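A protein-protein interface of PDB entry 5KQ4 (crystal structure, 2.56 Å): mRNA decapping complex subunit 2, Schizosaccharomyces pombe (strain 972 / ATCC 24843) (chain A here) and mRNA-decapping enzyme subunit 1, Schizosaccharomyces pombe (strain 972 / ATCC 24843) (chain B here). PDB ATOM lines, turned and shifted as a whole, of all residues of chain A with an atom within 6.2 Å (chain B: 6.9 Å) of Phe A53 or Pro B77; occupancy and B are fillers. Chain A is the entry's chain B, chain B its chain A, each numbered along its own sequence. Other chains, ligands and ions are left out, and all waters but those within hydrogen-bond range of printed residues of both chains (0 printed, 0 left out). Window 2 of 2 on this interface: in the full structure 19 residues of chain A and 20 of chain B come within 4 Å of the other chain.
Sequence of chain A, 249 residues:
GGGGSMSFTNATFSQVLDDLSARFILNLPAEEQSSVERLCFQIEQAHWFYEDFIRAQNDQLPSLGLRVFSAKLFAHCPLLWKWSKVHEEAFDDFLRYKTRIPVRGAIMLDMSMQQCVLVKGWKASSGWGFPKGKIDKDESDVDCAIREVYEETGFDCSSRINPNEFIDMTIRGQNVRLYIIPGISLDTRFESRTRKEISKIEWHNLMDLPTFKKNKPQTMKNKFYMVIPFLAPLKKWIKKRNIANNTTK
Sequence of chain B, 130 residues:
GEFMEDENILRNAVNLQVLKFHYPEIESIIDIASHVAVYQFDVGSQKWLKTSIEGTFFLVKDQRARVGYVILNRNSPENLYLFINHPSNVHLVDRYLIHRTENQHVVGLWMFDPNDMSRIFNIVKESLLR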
ATOM      1  N   GLY A   3      14.941  -2.609 -10.893  1.00  0.00           N
ATOM      2  CA  GLY A   3      13.848  -1.660 -11.017  1.00  0.00           C
ATOM      3  C   GLY A   3      13.426  -1.401 -12.452  1.00  0.00           C
ATOM      4  O   GLY A   3      13.040  -2.321 -13.171  1.00  0.00           O
ATOM      5  N   GLY A   4      13.489  -0.140 -12.869  1.00  0.00           N
ATOM      6  CA  GLY A   4      13.163   0.222 -14.234  1.00  0.00           C
ATOM      7  C   GLY A   4      13.958   1.418 -14.710  1.00  0.00           C
ATOM      8  O   GLY A   4      13.535   2.140 -15.618  1.00  0.00           O
ATOM      9  N   SER A   5      15.124   1.627 -14.102  1.00  0.00           N
ATOM     10  CA  SER A   5      15.927   2.818 -14.336  1.00  0.00           C
ATOM     11  C   SER A   5      16.699   2.777 -15.650  1.00  0.00           C
ATOM     12  O   SER A   5      17.362   3.765 -15.990  1.00  0.00           O
ATOM     13  CB  SER A   5      16.894   3.027 -13.169  1.00  0.00           C
ATOM     14  OG  SER A   5      17.347   4.368 -13.131  1.00  0.00           O
ATOM     15  N   SER A   7      14.960   1.763 -18.550  1.00  0.00           N
ATOM     16  CA  SER A   7      13.905   1.411 -19.493  1.00  0.00           C
ATOM     17  C   SER A   7      13.809   2.398 -20.650  1.00  0.00           C
ATOM     18  O   SER A   7      13.354   2.026 -21.737  1.00  0.00           O
ATOM     19  CB  SER A   7      12.567   1.308 -18.757  1.00  0.00           C
ATOM     20  OG  SER A   7      12.444   2.313 -17.762  1.00  0.00           O
ATOM     21  N   PHE A   8      14.235   3.647 -20.450  1.00  0.00           N
ATOM     22  CA  PHE A   8      14.080   4.691 -21.457  1.00  0.00           C
ATOM     23  C   PHE A   8      15.410   5.256 -21.950  1.00  0.00           C
ATOM     24  O   PHE A   8      15.408   6.238 -22.704  1.00  0.00           O
ATOM     25  CB  PHE A   8      13.220   5.832 -20.907  1.00  0.00           C
ATOM     26  CG  PHE A   8      11.851   5.405 -20.450  1.00  0.00           C
ATOM     27  CD1 PHE A   8      10.829   5.222 -21.364  1.00  0.00           C
ATOM     28  CD2 PHE A   8      11.586   5.201 -19.107  1.00  0.00           C
ATOM     29  CE1 PHE A   8       9.567   4.837 -20.948  1.00  0.00           C
ATOM     30  CE2 PHE A   8      10.325   4.814 -18.684  1.00  0.00           C
ATOM     31  CZ  PHE A   8       9.315   4.633 -19.608  1.00  0.00           C
ATOM     32  N   ARG A  23       0.489   4.460 -20.870  1.00  0.00           N
ATOM     33  CA  ARG A  23       0.665   4.466 -19.422  1.00  0.00           C
ATOM     34  C   ARG A  23      -0.374   5.320 -18.702  1.00  0.00           C
ATOM     35  O   ARG A  23      -0.675   5.057 -17.530  1.00  0.00           O
ATOM     36  CB  ARG A  23       2.070   4.961 -19.080  1.00  0.00           C
ATOM     37  CG  ARG A  23       2.684   4.320 -17.848  1.00  0.00           C
ATOM     38  CD  ARG A  23       4.136   4.744 -17.683  1.00  0.00           C
ATOM     39  NE  ARG A  23       4.884   3.881 -16.767  1.00  0.00           N
ATOM     40  CZ  ARG A  23       5.671   2.880 -17.150  1.00  0.00           C
ATOM     41  NH1 ARG A  23       5.815   2.608 -18.438  1.00  0.00           N
ATOM     42  NH2 ARG A  23       6.312   2.150 -16.245  1.00  0.00           N
ATOM     43  N   TRP A  48       4.518  14.895 -15.562  1.00  0.00           N
ATOM     44  CA  TRP A  48       5.354  14.710 -14.381  1.00  0.00           C
ATOM     45  C   TRP A  48       6.239  13.480 -14.526  1.00  0.00           C
ATOM     46  O   TRP A  48       7.436  13.519 -14.210  1.00  0.00           O
ATOM     47  CB  TRP A  48       4.472  14.596 -13.136  1.00  0.00           C
ATOM     48  CG  TRP A  48       3.787  15.872 -12.763  1.00  0.00           C
ATOM     49  CD1 TRP A  48       4.013  17.108 -13.293  1.00  0.00           C
ATOM     50  CD2 TRP A  48       2.761  16.040 -11.777  1.00  0.00           C
ATOM     51  NE1 TRP A  48       3.191  18.038 -12.699  1.00  0.00           N
ATOM     52  CE2 TRP A  48       2.414  17.405 -11.763  1.00  0.00           C
ATOM     53  CE3 TRP A  48       2.103  15.169 -10.904  1.00  0.00           C
ATOM     54  CZ2 TRP A  48       1.437  17.918 -10.911  1.00  0.00           C
ATOM     55  CZ3 TRP A  48       1.133  15.681 -10.059  1.00  0.00           C
ATOM     56  CH2 TRP A  48       0.812  17.043 -10.069  1.00  0.00           C
ATOM     57  N   PHE A  49       5.659  12.373 -14.999  1.00  0.00           N
ATOM     58  CA  PHE A  49       6.438  11.161 -15.235  1.00  0.00           C
ATOM     59  C   PHE A  49       7.566  11.426 -16.225  1.00  0.00           C
ATOM     60  O   PHE A  49       8.713  11.017 -16.005  1.00  0.00           O
ATOM     61  CB  PHE A  49       5.515  10.053 -15.747  1.00  0.00           C
ATOM     62  CG  PHE A  49       6.149   8.691 -15.779  1.00  0.00           C
ATOM     63  CD1 PHE A  49       6.074   7.858 -14.676  1.00  0.00           C
ATOM     64  CD2 PHE A  49       6.805   8.233 -16.914  1.00  0.00           C
ATOM     65  CE1 PHE A  49       6.650   6.599 -14.695  1.00  0.00           C
ATOM     66  CE2 PHE A  49       7.384   6.970 -16.939  1.00  0.00           C
ATOM     67  CZ  PHE A  49       7.305   6.154 -15.828  1.00  0.00           C
ATOM     68  N   TYR A  50       7.253  12.117 -17.325  1.00  0.00           N
ATOM     69  CA  TYR A  50       8.260  12.417 -18.339  1.00  0.00           C
ATOM     70  C   TYR A  50       9.403  13.242 -17.764  1.00  0.00           C
ATOM     71  O   TYR A  50      10.575  12.999 -18.075  1.00  0.00           O
ATOM     72  CB  TYR A  50       7.596  13.145 -19.510  1.00  0.00           C
ATOM     73  CG  TYR A  50       8.553  13.758 -20.508  1.00  0.00           C
ATOM     74  CD1 TYR A  50       9.076  13.005 -21.552  1.00  0.00           C
ATOM     75  CD2 TYR A  50       8.916  15.096 -20.420  1.00  0.00           C
ATOM     76  CE1 TYR A  50       9.948  13.564 -22.471  1.00  0.00           C
ATOM     77  CE2 TYR A  50       9.784  15.663 -21.333  1.00  0.00           C
ATOM     78  CZ  TYR A  50      10.298  14.891 -22.354  1.00  0.00           C
ATOM     79  OH  TYR A  50      11.164  15.449 -23.266  1.00  0.00           O
ATOM     80  N   GLU A  51       9.082  14.219 -16.911  1.00  0.00           N
ATOM     81  CA  GLU A  51      10.097  15.136 -16.407  1.00  0.00           C
ATOM     82  C   GLU A  51      10.939  14.506 -15.304  1.00  0.00           C
ATOM     83  O   GLU A  51      12.155  14.717 -15.251  1.00  0.00           O
ATOM     84  CB  GLU A  51       9.431  16.418 -15.899  1.00  0.00           C
ATOM     85  CG  GLU A  51      10.399  17.464 -15.365  1.00  0.00           C
ATOM     86  CD  GLU A  51      11.401  17.917 -16.404  1.00  0.00           C
ATOM     87  OE1 GLU A  51      12.593  18.066 -16.060  1.00  0.00           O
ATOM     88  OE2 GLU A  51      10.999  18.120 -17.568  1.00  0.00           O
ATOM     89  N   ASP A  52      10.315  13.728 -14.421  1.00  0.00           N
ATOM     90  CA  ASP A  52      11.009  13.195 -13.254  1.00  0.00           C
ATOM     91  C   ASP A  52      11.724  11.880 -13.521  1.00  0.00           C
ATOM     92  O   ASP A  52      12.774  11.627 -12.919  1.00  0.00           O
ATOM     93  CB  ASP A  52      10.020  12.995 -12.104  1.00  0.00           C
ATOM     94  CG  ASP A  52       9.348  14.281 -11.682  1.00  0.00           C
ATOM     95  OD1 ASP A  52       9.952  15.359 -11.856  1.00  0.00           O
ATOM     96  OD2 ASP A  52       8.211  14.212 -11.170  1.00  0.00           O
ATOM     97  N   PHE A  53      11.187  11.031 -14.395  1.00  0.00           N
ATOM     98  CA  PHE A  53      11.729   9.691 -14.587  1.00  0.00           C
ATOM     99  C   PHE A  53      12.298   9.474 -15.978  1.00  0.00           C
ATOM    100  O   PHE A  53      13.447   9.035 -16.107  1.00  0.00           O
ATOM    101  CB  PHE A  53      10.651   8.637 -14.294  1.00  0.00           C
ATOM    102  CG  PHE A  53      10.314   8.505 -12.839  1.00  0.00           C
ATOM    103  CD1 PHE A  53      11.245   8.002 -11.940  1.00  0.00           C
ATOM    104  CD2 PHE A  53       9.069   8.877 -12.366  1.00  0.00           C
ATOM    105  CE1 PHE A  53      10.937   7.874 -10.596  1.00  0.00           C
ATOM    106  CE2 PHE A  53       8.752   8.752 -11.025  1.00  0.00           C
ATOM    107  CZ  PHE A  53       9.688   8.249 -10.138  1.00  0.00           C
ATOM    108  N   ILE A  54      11.526   9.765 -17.027  1.00  0.00           N
ATOM    109  CA  ILE A  54      11.991   9.484 -18.382  1.00  0.00           C
ATOM    110  C   ILE A  54      13.141  10.407 -18.770  1.00  0.00           C
ATOM    111  O   ILE A  54      13.961  10.056 -19.624  1.00  0.00           O
ATOM    112  CB  ILE A  54      10.819   9.569 -19.380  1.00  0.00           C
ATOM    113  CG1 ILE A  54       9.757   8.524 -19.024  1.00  0.00           C
ATOM    114  CG2 ILE A  54      11.298   9.338 -20.814  1.00  0.00           C
ATOM    115  CD1 ILE A  54       8.743   8.266 -20.116  1.00  0.00           C
ATOM    116  N   ARG A  55      13.235  11.585 -18.154  1.00  0.00           N
ATOM    117  CA  ARG A  55      14.350  12.485 -18.418  1.00  0.00           C
ATOM    118  C   ARG A  55      15.485  12.338 -17.412  1.00  0.00           C
ATOM    119  O   ARG A  55      16.552  12.926 -17.619  1.00  0.00           O
ATOM    120  CB  ARG A  55      13.859  13.938 -18.467  1.00  0.00           C
ATOM    121  CG  ARG A  55      13.780  14.486 -19.886  1.00  0.00           C
ATOM    122  CD  ARG A  55      13.033  15.808 -19.961  1.00  0.00           C
ATOM    123  NE  ARG A  55      13.553  16.790 -19.016  1.00  0.00           N
ATOM    124  CZ  ARG A  55      14.672  17.482 -19.195  1.00  0.00           C
ATOM    125  NH1 ARG A  55      15.063  18.358 -18.281  1.00  0.00           N
ATOM    126  NH2 ARG A  55      15.405  17.294 -20.284  1.00  0.00           N
ATOM    127  N   ALA A  56      15.282  11.578 -16.333  1.00  0.00           N
ATOM    128  CA  ALA A  56      16.411  11.126 -15.526  1.00  0.00           C
ATOM    129  C   ALA A  56      17.336  10.256 -16.362  1.00  0.00           C
ATOM    130  O   ALA A  56      18.542  10.509 -16.449  1.00  0.00           O
ATOM    131  CB  ALA A  56      15.909  10.373 -14.296  1.00  0.00           C
ATOM    132  N   GLN A  57      16.780   9.230 -16.992  1.00  0.00           N
ATOM    133  CA  GLN A  57      17.452   8.567 -18.093  1.00  0.00           C
ATOM    134  C   GLN A  57      17.389   9.455 -19.334  1.00  0.00           C
ATOM    135  O   GLN A  57      16.531  10.329 -19.449  1.00  0.00           O
ATOM    136  CB  GLN A  57      16.794   7.216 -18.378  1.00  0.00           C
ATOM    137  CG  GLN A  57      15.962   6.689 -17.211  1.00  0.00           C
ATOM    138  CD  GLN A  57      15.236   5.394 -17.523  1.00  0.00           C
ATOM    139  OE1 GLN A  57      15.393   4.820 -18.601  1.00  0.00           O
ATOM    140  NE2 GLN A  57      14.438   4.922 -16.572  1.00  0.00           N
ATOM    141  N   LYS A 221      15.023  12.755  -8.787  1.00  0.00           N
ATOM    142  CA  LYS A 221      14.599  13.978  -9.463  1.00  0.00           C
ATOM    143  C   LYS A 221      13.141  14.296  -9.167  1.00  0.00           C
ATOM    144  O   LYS A 221      12.753  15.468  -9.139  1.00  0.00           O
ATOM    145  CB  LYS A 221      14.821  13.857 -10.972  1.00  0.00           C
ATOM    146  CG  LYS A 221      14.587  15.157 -11.736  1.00  0.00           C
ATOM    147  CD  LYS A 221      14.875  15.014 -13.223  1.00  0.00           C
ATOM    148  CE  LYS A 221      14.692  16.342 -13.948  1.00  0.00           C
ATOM    149  NZ  LYS A 221      14.929  16.222 -15.415  1.00  0.00           N
ATOM    150  N   ASN A 222      12.323  13.269  -8.939  1.00  0.00           N
ATOM    151  CA  ASN A 222      10.937  13.492  -8.554  1.00  0.00           C
ATOM    152  C   ASN A 222      10.794  14.033  -7.138  1.00  0.00           C
ATOM    153  O   ASN A 222       9.678  14.373  -6.738  1.00  0.00           O
ATOM    154  CB  ASN A 222      10.138  12.195  -8.689  1.00  0.00           C
ATOM    155  CG  ASN A 222      10.617  11.114  -7.742  1.00  0.00           C
ATOM    156  OD1 ASN A 222      11.817  10.867  -7.616  1.00  0.00           O
ATOM    157  ND2 ASN A 222       9.678  10.467  -7.065  1.00  0.00           N
ATOM    158  N   HIS B  22       9.376  -2.722 -24.097  1.00  0.00           N
ATOM    159  CA  HIS B  22       9.945  -3.175 -22.833  1.00  0.00           C
ATOM    160  C   HIS B  22      10.203  -4.675 -22.827  1.00  0.00           C
ATOM    161  O   HIS B  22      11.162  -5.133 -22.195  1.00  0.00           O
ATOM    162  CB  HIS B  22       9.028  -2.790 -21.670  1.00  0.00           C
ATOM    163  CG  HIS B  22       8.858  -1.309 -21.490  1.00  0.00           C
ATOM    164  ND1 HIS B  22       9.885  -0.487 -21.076  1.00  0.00           N
ATOM    165  CD2 HIS B  22       7.780  -0.506 -21.658  1.00  0.00           C
ATOM    166  CE1 HIS B  22       9.448   0.758 -20.997  1.00  0.00           C
ATOM    167  NE2 HIS B  22       8.174   0.774 -21.346  1.00  0.00           N
ATOM    168  N   TYR B  23       9.376  -5.453 -23.521  1.00  0.00           N
ATOM    169  CA  TYR B  23       9.444  -6.912 -23.479  1.00  0.00           C
ATOM    170  C   TYR B  23       9.329  -7.433 -24.905  1.00  0.00           C
ATOM    171  O   TYR B  23       8.219  -7.682 -25.397  1.00  0.00           O
ATOM    172  CB  TYR B  23       8.357  -7.482 -22.566  1.00  0.00           C
ATOM    173  CG  TYR B  23       8.316  -6.813 -21.207  1.00  0.00           C
ATOM    174  CD1 TYR B  23       9.367  -6.951 -20.307  1.00  0.00           C
ATOM    175  CD2 TYR B  23       7.236  -6.020 -20.835  1.00  0.00           C
ATOM    176  CE1 TYR B  23       9.339  -6.333 -19.070  1.00  0.00           C
ATOM    177  CE2 TYR B  23       7.201  -5.397 -19.598  1.00  0.00           C
ATOM    178  CZ  TYR B  23       8.253  -5.556 -18.720  1.00  0.00           C
ATOM    179  OH  TYR B  23       8.215  -4.936 -17.491  1.00  0.00           O
ATOM    180  N   ASN B  73       3.658   0.644 -14.628  1.00  0.00           N
ATOM    181  CA  ASN B  73       3.558   1.401 -13.388  1.00  0.00           C
ATOM    182  C   ASN B  73       3.394   2.886 -13.685  1.00  0.00           C
ATOM    183  O   ASN B  73       4.116   3.450 -14.511  1.00  0.00           O
ATOM    184  CB  ASN B  73       4.800   1.168 -12.530  1.00  0.00           C
ATOM    185  CG  ASN B  73       4.616   1.614 -11.090  1.00  0.00           C
ATOM    186  OD1 ASN B  73       3.535   2.048 -10.696  1.00  0.00           O
ATOM    187  ND2 ASN B  73       5.679   1.508 -10.296  1.00  0.00           N
ATOM    188  N   ARG B  74       2.445   3.519 -12.995  1.00  0.00           N
ATOM    189  CA  ARG B  74       2.223   4.953 -13.110  1.00  0.00           C
ATOM    190  C   ARG B  74       3.045   5.762 -12.117  1.00  0.00           C
ATOM    191  O   ARG B  74       3.120   6.988 -12.260  1.00  0.00           O
ATOM    192  CB  ARG B  74       0.739   5.277 -12.897  1.00  0.00           C
ATOM    193  CG  ARG B  74      -0.207   4.769 -13.974  1.00  0.00           C
ATOM    194  CD  ARG B  74      -1.650   5.042 -13.574  1.00  0.00           C
ATOM    195  NE  ARG B  74      -2.617   4.464 -14.503  1.00  0.00           N
ATOM    196  CZ  ARG B  74      -3.270   5.161 -15.427  1.00  0.00           C
ATOM    197  NH1 ARG B  74      -3.061   6.464 -15.544  1.00  0.00           N
ATOM    198  NH2 ARG B  74      -4.136   4.559 -16.230  1.00  0.00           N
ATOM    199  N   ASN B  75       3.668   5.116 -11.128  1.00  0.00           N
ATOM    200  CA  ASN B  75       4.405   5.821 -10.087  1.00  0.00           C
ATOM    201  C   ASN B  75       5.911   5.834 -10.315  1.00  0.00           C
ATOM    202  O   ASN B  75       6.605   6.671  -9.725  1.00  0.00           O
ATOM    203  CB  ASN B  75       4.106   5.194  -8.721  1.00  0.00           C
ATOM    204  CG  ASN B  75       2.623   5.201  -8.389  1.00  0.00           C
ATOM    205  OD1 ASN B  75       1.905   6.139  -8.731  1.00  0.00           O
ATOM    206  ND2 ASN B  75       2.157   4.144  -7.728  1.00  0.00           N
ATOM    207  N   SER B  76       6.420   4.940 -11.154  1.00  0.00           N
ATOM    208  CA  SER B  76       7.847   4.812 -11.413  1.00  0.00           C
ATOM    209  C   SER B  76       8.021   3.941 -12.654  1.00  0.00           C
ATOM    210  O   SER B  76       7.077   3.266 -13.069  1.00  0.00           O
ATOM    211  CB  SER B  76       8.586   4.191 -10.211  1.00  0.00           C
ATOM    212  OG  SER B  76       8.644   2.781 -10.323  1.00  0.00           O
ATOM    213  N   PRO B  77       9.208   3.948 -13.268  1.00  0.00           N
ATOM    214  CA  PRO B  77       9.437   3.092 -14.444  1.00  0.00           C
ATOM    215  C   PRO B  77       9.507   1.603 -14.129  1.00  0.00           C
ATOM    216  O   PRO B  77       9.654   0.796 -15.053  1.00  0.00           O
ATOM    217  CB  PRO B  77      10.784   3.597 -14.992  1.00  0.00           C
ATOM    218  CG  PRO B  77      11.003   4.935 -14.356  1.00  0.00           C
ATOM    219  CD  PRO B  77      10.333   4.868 -13.030  1.00  0.00           C
ATOM    220  N   GLU B  78       9.419   1.220 -12.860  1.00  0.00           N
ATOM    221  CA  GLU B  78       9.488  -0.181 -12.462  1.00  0.00           C
ATOM    222  C   GLU B  78       8.159  -0.863 -12.763  1.00  0.00           C
ATOM    223  O   GLU B  78       7.178  -0.664 -12.041  1.00  0.00           O
ATOM    224  CB  GLU B  78       9.832  -0.292 -10.980  1.00  0.00           C
ATOM    225  CG  GLU B  78       9.676  -1.695 -10.419  1.00  0.00           C
ATOM    226  CD  GLU B  78       9.678  -1.722  -8.907  1.00  0.00           C
ATOM    227  OE1 GLU B  78       9.858  -2.814  -8.332  1.00  0.00           O
ATOM    228  OE2 GLU B  78       9.501  -0.650  -8.291  1.00  0.00           O
ATOM    229  N   ASN B  79       8.128  -1.679 -13.816  1.00  0.00           N
ATOM    230  CA  ASN B  79       6.930  -2.417 -14.172  1.00  0.00           C
ATOM    231  C   ASN B  79       6.942  -3.794 -13.507  1.00  0.00           C
ATOM    232  O   ASN B  79       7.912  -4.194 -12.856  1.00  0.00           O
ATOM    233  CB  ASN B  79       6.816  -2.557 -15.688  1.00  0.00           C
ATOM    234  CG  ASN B  79       6.908  -1.230 -16.410  1.00  0.00           C
ATOM    235  OD1 ASN B  79       6.146  -0.302 -16.135  1.00  0.00           O
ATOM    236  ND2 ASN B  79       7.846  -1.134 -17.344  1.00  0.00           N
ATOM    237  N   LEU B  80       5.841  -4.527 -13.664  1.00  0.00           N
ATOM    238  CA  LEU B  80       5.730  -5.891 -13.162  1.00  0.00           C
ATOM    239  C   LEU B  80       5.321  -6.796 -14.311  1.00  0.00           C
ATOM    240  O   LEU B  80       4.307  -6.546 -14.969  1.00  0.00           O
ATOM    241  CB  LEU B  80       4.722  -5.993 -12.015  1.00  0.00           C
ATOM    242  CG  LEU B  80       4.665  -7.377 -11.363  1.00  0.00           C
ATOM    243  CD1 LEU B  80       6.019  -7.749 -10.761  1.00  0.00           C
ATOM    244  CD2 LEU B  80       3.571  -7.428 -10.309  1.00  0.00           C
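O of Asn B73 is in hydrogen-bond range of NE of Arg A23, at 2.4 Å. The guanidinium group (NH1) of Arg B74 lies close to the backbone carbonyl oxygen (O) of Arg A23 (3.4 Å). O of Ser B76 is in hydrogen-bond range of NH2 of Arg A23. The side-chain amide oxygen (OD1) of Asn B79 sits at hydrogen-bond distance from the guanidinium group (NH2) of Arg A23, at 2.5 Å.
The side-chain amide oxygen (OD1) of Asn B73 lies within hydrogen-bond range of the backbone NH (N) of Asn B75, 3.1 Å away. The side-chain amide nitrogen (ND2) of Asn B79 is in hydrogen-bond range of the backbone carbonyl oxygen (O) of Pro B77 (3.5 Å). The side-chain hydroxyl (OG) of Ser A7 sits at hydrogen-bond distance from the backbone carbonyl oxygen (O) of Gly A4, 2.4 Å away. The side-chain amide nitrogen (NE2) of Gln A57 sits at hydrogen-bond distance from the backbone carbonyl oxygen (O) of Gly A4, 3.1 Å away. N of Phe A8 lies within hydrogen-bond range of OE1 of Gln A57 (2.5 Å). The backbone NH (N) of Ile A54 lies within hydrogen-bond range of the backbone carbonyl oxygen (O) of Phe A49 (3.2 Å).
Along chain B the printed residues that touch a printed residue of chain A span positions 22 to 79. Of the 18 printed residues of chain A, 6 touch a printed residue of chain B. Hydrophobic or aromatic side chains of chain A within 4 Å of the printed part of chain B: Phe A8, Phe A49 and Phe A53. Among the printed residues, no Asp or Glu carboxylate lies within 4 Å of a Lys or Arg side-chain nitrogen of the other chain.
Printed residues of chain B within 4 Å of Arg A23: Asn B73, Arg B74, Ser B76, Pro B77 and Asn B79. Of the printed residues of chain B, Phe A53 touches Asn B75 (3.3 Å) and Pro B77 (3.4 Å). Lys A221 touches none of the printed residues of chain B. Printed residues of chain A within 4 Å of His B22: Ser A7. Of the printed residues of chain A, Asn B73 touches Arg A23 (2.4 Å). Printed residues of chain A within 4 Å of Ser B76: Arg A23 (3.5 Å) and Phe A49 (3.6 Å). Of chain A, only Gly A4 (3.2 Å), Ser A7 (3.5 Å), Phe A8 (3.9 Å), Arg A23 (3.7 Å), Phe A49 (3.9 Å) and Phe A53 (3.4 Å) come within 4 Å of Pro B77. The nearest residue of chain B that does not touch Phe A53 is Ser B76 (4.1 Å). The nearest residue of chain A that does not touch Pro B77 is Gln A57 (4.1 Å).
Among the printed residues, merely in contact across the chains: Gly A4 with Pro B77 (3.2 Å), Ser A7 with His B22 (3.9 Å), Ser A7 with Pro B77 (3.5 Å), Phe A8 with Pro B77 (3.9 Å), Arg A23 with Pro B77 (3.7 Å), Phe A49 with Arg B74 (3.9 Å), Phe A49 with Ser B76 (3.6 Å), Phe A49 with Pro B77 (3.9 Å), Phe A53 with Asn B75 (3.3 Å) and Phe A53 with Pro B77 (3.4 Å).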
